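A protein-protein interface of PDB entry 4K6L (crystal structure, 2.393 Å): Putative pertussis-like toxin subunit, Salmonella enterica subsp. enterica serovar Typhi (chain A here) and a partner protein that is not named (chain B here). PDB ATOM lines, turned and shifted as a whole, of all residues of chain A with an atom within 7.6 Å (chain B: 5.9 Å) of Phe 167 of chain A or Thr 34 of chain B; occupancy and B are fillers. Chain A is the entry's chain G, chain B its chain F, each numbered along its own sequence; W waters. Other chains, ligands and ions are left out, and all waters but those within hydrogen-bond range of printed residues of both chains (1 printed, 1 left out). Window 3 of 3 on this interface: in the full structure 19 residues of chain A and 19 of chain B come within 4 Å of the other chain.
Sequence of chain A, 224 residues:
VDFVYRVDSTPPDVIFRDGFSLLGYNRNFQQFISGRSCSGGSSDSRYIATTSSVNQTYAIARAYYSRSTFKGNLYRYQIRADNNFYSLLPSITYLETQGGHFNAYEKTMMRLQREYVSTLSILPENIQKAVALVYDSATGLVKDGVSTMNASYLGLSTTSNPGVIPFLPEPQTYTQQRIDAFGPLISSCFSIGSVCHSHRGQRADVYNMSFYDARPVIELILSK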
ATOM      1  N   TYR A  25      16.379   4.158   2.636  1.00  0.00           N
ATOM      2  CA  TYR A  25      16.528   5.601   2.437  1.00  0.00           C
ATOM      3  C   TYR A  25      16.851   6.016   0.985  1.00  0.00           C
ATOM      4  O   TYR A  25      17.143   7.183   0.714  1.00  0.00           O
ATOM      5  CB  TYR A  25      17.617   6.153   3.367  1.00  0.00           C
ATOM      6  CG  TYR A  25      17.344   6.006   4.855  1.00  0.00           C
ATOM      7  CD1 TYR A  25      16.249   6.626   5.450  1.00  0.00           C
ATOM      8  CD2 TYR A  25      18.204   5.277   5.671  1.00  0.00           C
ATOM      9  CE1 TYR A  25      16.004   6.504   6.807  1.00  0.00           C
ATOM     10  CE2 TYR A  25      17.970   5.150   7.035  1.00  0.00           C
ATOM     11  CZ  TYR A  25      16.869   5.767   7.597  1.00  0.00           C
ATOM     12  OH  TYR A  25      16.632   5.649   8.950  1.00  0.00           O
ATOM     13  N   ASN A  26      16.809   5.070   0.055  1.00  0.00           N
ATOM     14  CA  ASN A  26      17.127   5.374  -1.337  1.00  0.00           C
ATOM     15  C   ASN A  26      16.016   6.178  -2.025  1.00  0.00           C
ATOM     16  O   ASN A  26      14.954   5.643  -2.334  1.00  0.00           O
ATOM     17  CB  ASN A  26      17.430   4.082  -2.100  1.00  0.00           C
ATOM     18  CG  ASN A  26      17.954   4.332  -3.509  1.00  0.00           C
ATOM     19  OD1 ASN A  26      18.059   5.475  -3.958  1.00  0.00           O
ATOM     20  ND2 ASN A  26      18.300   3.253  -4.206  1.00  0.00           N
ATOM     21  N   ARG A  27      16.281   7.460  -2.262  1.00  0.00           N
ATOM     22  CA  ARG A  27      15.295   8.382  -2.823  1.00  0.00           C
ATOM     23  C   ARG A  27      15.232   8.354  -4.347  1.00  0.00           C
ATOM     24  O   ARG A  27      14.341   8.964  -4.937  1.00  0.00           O
ATOM     25  CB  ARG A  27      15.610   9.822  -2.418  1.00  0.00           C
ATOM     26  CG  ARG A  27      15.593  10.146  -0.932  1.00  0.00           C
ATOM     27  CD  ARG A  27      15.754  11.655  -0.778  1.00  0.00           C
ATOM     28  NE  ARG A  27      16.144  12.071   0.565  1.00  0.00           N
ATOM     29  CZ  ARG A  27      15.287  12.353   1.539  1.00  0.00           C
ATOM     30  NH1 ARG A  27      13.984  12.251   1.330  1.00  0.00           N
ATOM     31  NH2 ARG A  27      15.736  12.732   2.723  1.00  0.00           N
ATOM     32  N   ASN A  28      16.187   7.676  -4.979  1.00  0.00           N
ATOM     33  CA  ASN A  28      16.308   7.705  -6.435  1.00  0.00           C
ATOM     34  C   ASN A  28      15.021   7.258  -7.118  1.00  0.00           C
ATOM     35  O   ASN A  28      14.597   6.109  -6.985  1.00  0.00           O
ATOM     36  CB  ASN A  28      17.494   6.860  -6.898  1.00  0.00           C
ATOM     37  CG  ASN A  28      17.863   7.113  -8.340  1.00  0.00           C
ATOM     38  OD1 ASN A  28      16.998   7.273  -9.204  1.00  0.00           O
ATOM     39  ND2 ASN A  28      19.157   7.148  -8.612  1.00  0.00           N
ATOM     40  N   ARG A  46      13.050   4.253  -0.600  1.00  0.00           N
ATOM     41  CA  ARG A  46      12.431   5.141   0.377  1.00  0.00           C
ATOM     42  C   ARG A  46      11.020   5.518  -0.065  1.00  0.00           C
ATOM     43  O   ARG A  46      10.549   6.627   0.192  1.00  0.00           O
ATOM     44  CB  ARG A  46      13.275   6.405   0.529  1.00  0.00           C
ATOM     45  CG  ARG A  46      13.069   7.170   1.824  1.00  0.00           C
ATOM     46  CD  ARG A  46      14.110   8.260   1.923  1.00  0.00           C
ATOM     47  NE  ARG A  46      14.101   8.918   3.219  1.00  0.00           N
ATOM     48  CZ  ARG A  46      15.151   9.546   3.733  1.00  0.00           C
ATOM     49  NH1 ARG A  46      16.295   9.592   3.059  1.00  0.00           N
ATOM     50  NH2 ARG A  46      15.059  10.117   4.927  1.00  0.00           N
ATOM     51  N   TYR A  47      10.358   4.595  -0.757  1.00  0.00           N
ATOM     52  CA  TYR A  47       8.974   4.793  -1.165  1.00  0.00           C
ATOM     53  C   TYR A  47       8.195   3.493  -1.010  1.00  0.00           C
ATOM     54  O   TYR A  47       8.771   2.409  -1.006  1.00  0.00           O
ATOM     55  CB  TYR A  47       8.886   5.252  -2.628  1.00  0.00           C
ATOM     56  CG  TYR A  47       9.752   6.443  -2.993  1.00  0.00           C
ATOM     57  CD1 TYR A  47       9.356   7.744  -2.682  1.00  0.00           C
ATOM     58  CD2 TYR A  47      10.956   6.268  -3.674  1.00  0.00           C
ATOM     59  CE1 TYR A  47      10.142   8.834  -3.027  1.00  0.00           C
ATOM     60  CE2 TYR A  47      11.748   7.351  -4.022  1.00  0.00           C
ATOM     61  CZ  TYR A  47      11.338   8.630  -3.697  1.00  0.00           C
ATOM     62  OH  TYR A  47      12.129   9.707  -4.041  1.00  0.00           O
ATOM     63  N   TYR A  86       1.972  10.402  -3.927  1.00  0.00           N
ATOM     64  CA  TYR A  86       2.183  11.137  -5.168  1.00  0.00           C
ATOM     65  C   TYR A  86       2.004  10.240  -6.378  1.00  0.00           C
ATOM     66  O   TYR A  86       2.385   9.071  -6.349  1.00  0.00           O
ATOM     67  CB  TYR A  86       3.598  11.720  -5.204  1.00  0.00           C
ATOM     68  CG  TYR A  86       3.911  12.702  -4.104  1.00  0.00           C
ATOM     69  CD1 TYR A  86       4.197  12.265  -2.809  1.00  0.00           C
ATOM     70  CD2 TYR A  86       3.948  14.065  -4.357  1.00  0.00           C
ATOM     71  CE1 TYR A  86       4.493  13.163  -1.799  1.00  0.00           C
ATOM     72  CE2 TYR A  86       4.249  14.970  -3.352  1.00  0.00           C
ATOM     73  CZ  TYR A  86       4.514  14.515  -2.074  1.00  0.00           C
ATOM     74  OH  TYR A  86       4.807  15.414  -1.072  1.00  0.00           O
ATOM     75  N   TYR A  94       9.082  16.623 -14.045  1.00  0.00           N
ATOM     76  CA  TYR A  94      10.068  17.500 -13.411  1.00  0.00           C
ATOM     77  C   TYR A  94      11.502  17.049 -13.674  1.00  0.00           C
ATOM     78  O   TYR A  94      12.346  17.846 -14.091  1.00  0.00           O
ATOM     79  CB  TYR A  94       9.854  17.593 -11.894  1.00  0.00           C
ATOM     80  CG  TYR A  94      10.988  18.323 -11.203  1.00  0.00           C
ATOM     81  CD1 TYR A  94      11.043  19.711 -11.209  1.00  0.00           C
ATOM     82  CD2 TYR A  94      12.017  17.625 -10.573  1.00  0.00           C
ATOM     83  CE1 TYR A  94      12.083  20.391 -10.600  1.00  0.00           C
ATOM     84  CE2 TYR A  94      13.067  18.299  -9.959  1.00  0.00           C
ATOM     85  CZ  TYR A  94      13.091  19.682  -9.979  1.00  0.00           C
ATOM     86  OH  TYR A  94      14.119  20.368  -9.378  1.00  0.00           O
ATOM     87  N   THR A 119       5.837   8.608   0.450  1.00  0.00           N
ATOM     88  CA  THR A 119       7.184   9.010   0.837  1.00  0.00           C
ATOM     89  C   THR A 119       7.512   8.642   2.280  1.00  0.00           C
ATOM     90  O   THR A 119       8.678   8.616   2.678  1.00  0.00           O
ATOM     91  CB  THR A 119       7.405  10.523   0.635  1.00  0.00           C
ATOM     92  OG1 THR A 119       6.402  11.258   1.346  1.00  0.00           O
ATOM     93  CG2 THR A 119       7.335  10.869  -0.838  1.00  0.00           C
ATOM     94  N   VAL A 164       4.833  17.431  -7.112  1.00  0.00           N
ATOM     95  CA  VAL A 164       6.086  16.721  -7.320  1.00  0.00           C
ATOM     96  C   VAL A 164       6.667  16.225  -6.003  1.00  0.00           C
ATOM     97  O   VAL A 164       6.700  16.958  -5.015  1.00  0.00           O
ATOM     98  CB  VAL A 164       7.122  17.635  -8.007  1.00  0.00           C
ATOM     99  CG1 VAL A 164       8.455  16.919  -8.169  1.00  0.00           C
ATOM    100  CG2 VAL A 164       6.599  18.113  -9.355  1.00  0.00           C
ATOM    101  N   ILE A 165       7.111  14.971  -5.998  1.00  0.00           N
ATOM    102  CA  ILE A 165       7.831  14.393  -4.871  1.00  0.00           C
ATOM    103  C   ILE A 165       9.007  15.286  -4.470  1.00  0.00           C
ATOM    104  O   ILE A 165       9.818  15.675  -5.316  1.00  0.00           O
ATOM    105  CB  ILE A 165       8.341  12.982  -5.226  1.00  0.00           C
ATOM    106  CG1 ILE A 165       7.183  12.118  -5.733  1.00  0.00           C
ATOM    107  CG2 ILE A 165       9.028  12.327  -4.036  1.00  0.00           C
ATOM    108  CD1 ILE A 165       7.621  10.807  -6.355  1.00  0.00           C
ATOM    109  N   PRO A 166       9.090  15.634  -3.178  1.00  0.00           N
ATOM    110  CA  PRO A 166      10.150  16.531  -2.705  1.00  0.00           C
ATOM    111  C   PRO A 166      11.477  15.804  -2.530  1.00  0.00           C
ATOM    112  O   PRO A 166      11.502  14.577  -2.432  1.00  0.00           O
ATOM    113  CB  PRO A 166       9.624  16.996  -1.350  1.00  0.00           C
ATOM    114  CG  PRO A 166       8.795  15.842  -0.866  1.00  0.00           C
ATOM    115  CD  PRO A 166       8.164  15.244  -2.098  1.00  0.00           C
ATOM    116  N   PHE A 167      12.568  16.561  -2.511  1.00  0.00           N
ATOM    117  CA  PHE A 167      13.896  16.013  -2.252  1.00  0.00           C
ATOM    118  C   PHE A 167      14.342  14.995  -3.308  1.00  0.00           C
ATOM    119  O   PHE A 167      15.152  14.115  -3.021  1.00  0.00           O
ATOM    120  CB  PHE A 167      13.954  15.387  -0.848  1.00  0.00           C
ATOM    121  CG  PHE A 167      13.233  16.188   0.205  1.00  0.00           C
ATOM    122  CD1 PHE A 167      13.464  17.548   0.343  1.00  0.00           C
ATOM    123  CD2 PHE A 167      12.315  15.582   1.043  1.00  0.00           C
ATOM    124  CE1 PHE A 167      12.798  18.287   1.303  1.00  0.00           C
ATOM    125  CE2 PHE A 167      11.646  16.318   2.008  1.00  0.00           C
ATOM    126  CZ  PHE A 167      11.889  17.672   2.135  1.00  0.00           C
ATOM    127  N   LEU A 168      13.818  15.110  -4.524  1.00  0.00           N
ATOM    128  CA  LEU A 168      14.230  14.209  -5.598  1.00  0.00           C
ATOM    129  C   LEU A 168      15.709  14.407  -5.934  1.00  0.00           C
ATOM    130  O   LEU A 168      16.181  15.540  -6.031  1.00  0.00           O
ATOM    131  CB  LEU A 168      13.368  14.410  -6.846  1.00  0.00           C
ATOM    132  CG  LEU A 168      11.951  13.827  -6.836  1.00  0.00           C
ATOM    133  CD1 LEU A 168      11.144  14.417  -7.972  1.00  0.00           C
ATOM    134  CD2 LEU A 168      11.975  12.314  -6.951  1.00  0.00           C
ATOM    135  N   PRO A 169      16.454  13.301  -6.069  1.00  0.00           N
ATOM    136  CA  PRO A 169      17.833  13.359  -6.566  1.00  0.00           C
ATOM    137  C   PRO A 169      17.843  13.675  -8.063  1.00  0.00           C
ATOM    138  O   PRO A 169      16.894  13.326  -8.764  1.00  0.00           O
ATOM    139  CB  PRO A 169      18.358  11.941  -6.314  1.00  0.00           C
ATOM    140  CG  PRO A 169      17.436  11.363  -5.264  1.00  0.00           C
ATOM    141  CD  PRO A 169      16.102  11.962  -5.564  1.00  0.00           C
ATOM    142  N   GLU A 170      18.903  14.323  -8.538  1.00  0.00           N
ATOM    143  CA  GLU A 170      18.967  14.813  -9.919  1.00  0.00           C
ATOM    144  C   GLU A 170      19.165  13.783 -11.054  1.00  0.00           C
ATOM    145  O   GLU A 170      18.400  13.799 -12.018  1.00  0.00           O
ATOM    146  CB  GLU A 170      20.002  15.943 -10.043  1.00  0.00           C
ATOM    147  CG  GLU A 170      19.793  17.108  -9.075  1.00  0.00           C
ATOM    148  CD  GLU A 170      18.627  18.011  -9.454  1.00  0.00           C
ATOM    149  OE1 GLU A 170      17.462  17.554  -9.407  1.00  0.00           O
ATOM    150  OE2 GLU A 170      18.879  19.188  -9.794  1.00  0.00           O
ATOM    151  N   LYS B   6      16.521  10.026   8.521  1.00  0.00           N
ATOM    152  CA  LYS B   6      17.858   9.836   9.053  1.00  0.00           C
ATOM    153  C   LYS B   6      18.001  10.809  10.209  1.00  0.00           C
ATOM    154  O   LYS B   6      18.031  12.021  10.011  1.00  0.00           O
ATOM    155  CB  LYS B   6      18.929  10.086   7.990  1.00  0.00           C
ATOM    156  CG  LYS B   6      18.978   9.028   6.895  1.00  0.00           C
ATOM    157  CD  LYS B   6      20.139   9.274   5.939  1.00  0.00           C
ATOM    158  CE  LYS B   6      20.140   8.259   4.817  1.00  0.00           C
ATOM    159  NZ  LYS B   6      21.333   8.382   3.937  1.00  0.00           N
ATOM    160  N   LEU B  31      24.649  17.197   7.052  1.00  0.00           N
ATOM    161  CA  LEU B  31      23.314  17.457   6.516  1.00  0.00           C
ATOM    162  C   LEU B  31      23.236  17.468   4.984  1.00  0.00           C
ATOM    163  O   LEU B  31      22.203  17.108   4.412  1.00  0.00           O
ATOM    164  CB  LEU B  31      22.779  18.781   7.064  1.00  0.00           C
ATOM    165  CG  LEU B  31      22.567  18.916   8.573  1.00  0.00           C
ATOM    166  CD1 LEU B  31      22.127  20.330   8.908  1.00  0.00           C
ATOM    167  CD2 LEU B  31      21.551  17.915   9.081  1.00  0.00           C
ATOM    168  N   SER B  32      24.324  17.876   4.332  1.00  0.00           N
ATOM    169  CA  SER B  32      24.325  18.120   2.888  1.00  0.00           C
ATOM    170  C   SER B  32      23.861  16.944   2.038  1.00  0.00           C
ATOM    171  O   SER B  32      24.061  15.786   2.398  1.00  0.00           O
ATOM    172  CB  SER B  32      25.709  18.581   2.418  1.00  0.00           C
ATOM    173  OG  SER B  32      25.976  19.901   2.862  1.00  0.00           O
ATOM    174  N   GLY B  33      23.238  17.263   0.903  1.00  0.00           N
ATOM    175  CA  GLY B  33      22.790  16.264  -0.051  1.00  0.00           C
ATOM    176  C   GLY B  33      21.469  15.624   0.326  1.00  0.00           C
ATOM    177  O   GLY B  33      20.972  15.802   1.438  1.00  0.00           O
ATOM    178  N   THR B  34      20.895  14.869  -0.605  1.00  0.00           N
ATOM    179  CA  THR B  34      19.638  14.183  -0.343  1.00  0.00           C
ATOM    180  C   THR B  34      19.847  13.029   0.634  1.00  0.00           C
ATOM    181  O   THR B  34      18.926  12.647   1.350  1.00  0.00           O
ATOM    182  CB  THR B  34      18.997  13.653  -1.636  1.00  0.00           C
ATOM    183  OG1 THR B  34      19.765  12.552  -2.137  1.00  0.00           O
ATOM    184  CG2 THR B  34      18.927  14.754  -2.686  1.00  0.00           C
ATOM    185  N   ALA B  35      21.061  12.484   0.660  1.00  0.00           N
ATOM    186  CA  ALA B  35      21.411  11.410   1.590  1.00  0.00           C
ATOM    187  C   ALA B  35      21.818  11.952   2.960  1.00  0.00           C
ATOM    188  O   ALA B  35      22.091  11.186   3.887  1.00  0.00           O
ATOM    189  CB  ALA B  35      22.524  10.548   1.016  1.00  0.00           C
ATOM    190  N   GLY B  36      21.856  13.274   3.084  1.00  0.00           N
ATOM    191  CA  GLY B  36      22.239  13.908   4.332  1.00  0.00           C
ATOM    192  C   GLY B  36      21.222  13.677   5.426  1.00  0.00           C
ATOM    193  O   GLY B  36      20.083  13.303   5.152  1.00  0.00           O
ATOM    194  N   ASP B  38      18.360  14.068   7.971  1.00  0.00           N
ATOM    195  CA  ASP B  38      17.112  14.823   7.867  1.00  0.00           C
ATOM    196  C   ASP B  38      16.783  15.569   9.148  1.00  0.00           C
ATOM    197  O   ASP B  38      16.372  16.725   9.106  1.00  0.00           O
ATOM    198  CB  ASP B  38      15.956  13.898   7.500  1.00  0.00           C
ATOM    199  CG  ASP B  38      16.290  13.005   6.338  1.00  0.00           C
ATOM    200  OD1 ASP B  38      16.416  13.530   5.212  1.00  0.00           O
ATOM    201  OD2 ASP B  38      16.439  11.784   6.552  1.00  0.00           O
ATOM    202  N   ASP B  82      18.976  24.442  -1.265  1.00  0.00           N
ATOM    203  CA  ASP B  82      18.570  23.346  -0.399  1.00  0.00           C
ATOM    204  C   ASP B  82      18.295  23.929   0.982  1.00  0.00           C
ATOM    205  O   ASP B  82      19.193  24.015   1.824  1.00  0.00           O
ATOM    206  CB  ASP B  82      19.665  22.276  -0.344  1.00  0.00           C
ATOM    207  CG  ASP B  82      19.303  21.099   0.547  1.00  0.00           C
ATOM    208  OD1 ASP B  82      18.138  21.005   0.990  1.00  0.00           O
ATOM    209  OD2 ASP B  82      20.193  20.257   0.796  1.00  0.00           O
ATOM    210  N   ARG B  84      17.023  24.216   4.695  1.00  0.00           N
ATOM    211  CA  ARG B  84      16.713  23.443   5.884  1.00  0.00           C
ATOM    212  C   ARG B  84      16.128  24.363   6.941  1.00  0.00           C
ATOM    213  O   ARG B  84      16.319  25.576   6.889  1.00  0.00           O
ATOM    214  CB  ARG B  84      17.959  22.750   6.436  1.00  0.00           C
ATOM    215  CG  ARG B  84      18.744  21.948   5.418  1.00  0.00           C
ATOM    216  CD  ARG B  84      17.952  20.815   4.799  1.00  0.00           C
ATOM    217  NE  ARG B  84      18.739  20.185   3.742  1.00  0.00           N
ATOM    218  CZ  ARG B  84      19.473  19.088   3.902  1.00  0.00           C
ATOM    219  NH1 ARG B  84      19.506  18.472   5.079  1.00  0.00           N
ATOM    220  NH2 ARG B  84      20.167  18.602   2.880  1.00  0.00           N
ATOM    221  N   ARG B 105      14.747  18.884   7.656  1.00  0.00           N
ATOM    222  CA  ARG B 105      14.717  19.014   6.206  1.00  0.00           C
ATOM    223  C   ARG B 105      13.411  19.681   5.778  1.00  0.00           C
ATOM    224  O   ARG B 105      13.281  20.147   4.651  1.00  0.00           O
ATOM    225  CB  ARG B 105      14.889  17.644   5.541  1.00  0.00           C
ATOM    226  CG  ARG B 105      15.136  17.689   4.040  1.00  0.00           C
ATOM    227  CD  ARG B 105      15.343  16.293   3.458  1.00  0.00           C
ATOM    228  NE  ARG B 105      16.678  15.758   3.732  1.00  0.00           N
ATOM    229  CZ  ARG B 105      17.726  15.898   2.922  1.00  0.00           C
ATOM    230  NH1 ARG B 105      17.604  16.566   1.782  1.00  0.00           N
ATOM    231  NH2 ARG B 105      18.901  15.376   3.247  1.00  0.00           N
ATOM    232  N   GLN B 106      12.447  19.733   6.692  1.00  0.00           N
ATOM    233  CA  GLN B 106      11.179  20.399   6.410  1.00  0.00           C
ATOM    234  C   GLN B 106      10.602  21.177   7.599  1.00  0.00           C
ATOM    235  O   GLN B 106      11.019  21.003   8.745  1.00  0.00           O
ATOM    236  CB  GLN B 106      10.154  19.413   5.844  1.00  0.00           C
ATOM    237  CG  GLN B 106      10.260  18.008   6.395  1.00  0.00           C
ATOM    238  CD  GLN B 106       9.504  17.000   5.549  1.00  0.00           C
ATOM    239  OE1 GLN B 106       8.568  17.353   4.831  1.00  0.00           O
ATOM    240  NE2 GLN B 106       9.913  15.738   5.625  1.00  0.00           N
HETATM  241  O   HOH W   1      18.691   9.286   1.059  1.00  0.00           O
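NE of Arg 27 of chain A sits at hydrogen-bond distance from O of Thr 34 of chain B, at 2.9 Å.
The side-chain carboxylate (OD2) of Asp 38 of chain B lies within salt-bridge range of the guanidinium group (NH2) of Arg 46 of chain A.
The guanidinium group (NH2) of Arg 27 of chain A is in salt-bridge range of the side-chain carboxylate (OD1) of Asp 38 of chain B, at 2.7 Å.
NH2 of Arg 27 of chain A sits close to NE of Arg 105 of chain B (3.3 Å).
O of Gly 33 of chain B is in hydrogen-bond range of NH2 of Arg 105 of chain B (2.8 Å).
The side-chain amino group (NZ) of Lys 6 of chain B is in hydrogen-bond range of the backbone carbonyl oxygen (O) of Ala 35 of chain B (2.9 Å).
The guanidinium group of Arg 105 of chain B is in salt-bridge range of the side-chain carboxylate of Asp 38 of chain B.
The backbone carbonyl oxygen (O) of Thr 34 of chain B lies within hydrogen-bond range of the guanidinium group (NH2) of Arg 105 of chain B, at 3.3 Å.
OD2 of Asp 38 of chain B lies within hydrogen-bond range of N of Lys 6 of chain B (2.6 Å).
NH1 of Arg 46 of chain A lies close to O of Tyr 25 of chain A, at 3.5 Å.
Among the printed residues, merely in contact across the chains: Tyr 25 of chain A with Lys 6 of chain B, Arg 46 of chain A with Lys 6 of chain B, Phe 167 of chain A with Thr 34 of chain B and Phe 167 of chain A with Arg 105 of chain B.
Printed residues of chain B within 4 Å of Phe 167 of chain A: Thr 34 (3.8 Å) and Arg 105 (3.6 Å).
Of the printed residues of chain A, Thr 34 of chain B touches Arg 27 (2.9 Å) and Phe 167 (3.8 Å).
Of the printed residues of chain B, Arg 27 of chain A touches Thr 34, Asp 38 and Arg 105.
Of the printed residues of chain A, Arg 105 of chain B touches Arg 27 (3.3 Å) and Phe 167 (3.6 Å).
Of the printed residues of chain A, Asp 38 of chain B touches Arg 27 (2.7 Å) and Arg 46 (2.7 Å).
Asn 28 of chain A touches none of the printed residues of chain B.
Gly 36 of chain B touches none of the printed residues of chain A.
The nearest residue of chain B that does not touch Phe 167 of chain A is Gln 106 of chain B (4.1 Å).
Hydrophobic or aromatic side chains of chain A within 4 Å of the printed part of chain B: Tyr 25 and Phe 167.
Among the printed residues, Asp or Glu carboxylates within 4 Å of a Lys or Arg side-chain nitrogen of the other chain: Arg 27 of chain A with Asp 38 of chain B (2.7 Å) and Arg 46 of chain A with Asp 38 of chain B (2.7 Å).
Water W1 lies within hydrogen-bond range of O of Tyr 25 of chain A (2.6 Å), NH1 of Arg 46 of chain A (3.1 Å) and O of Thr 34 of chain B (3.4 Å).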
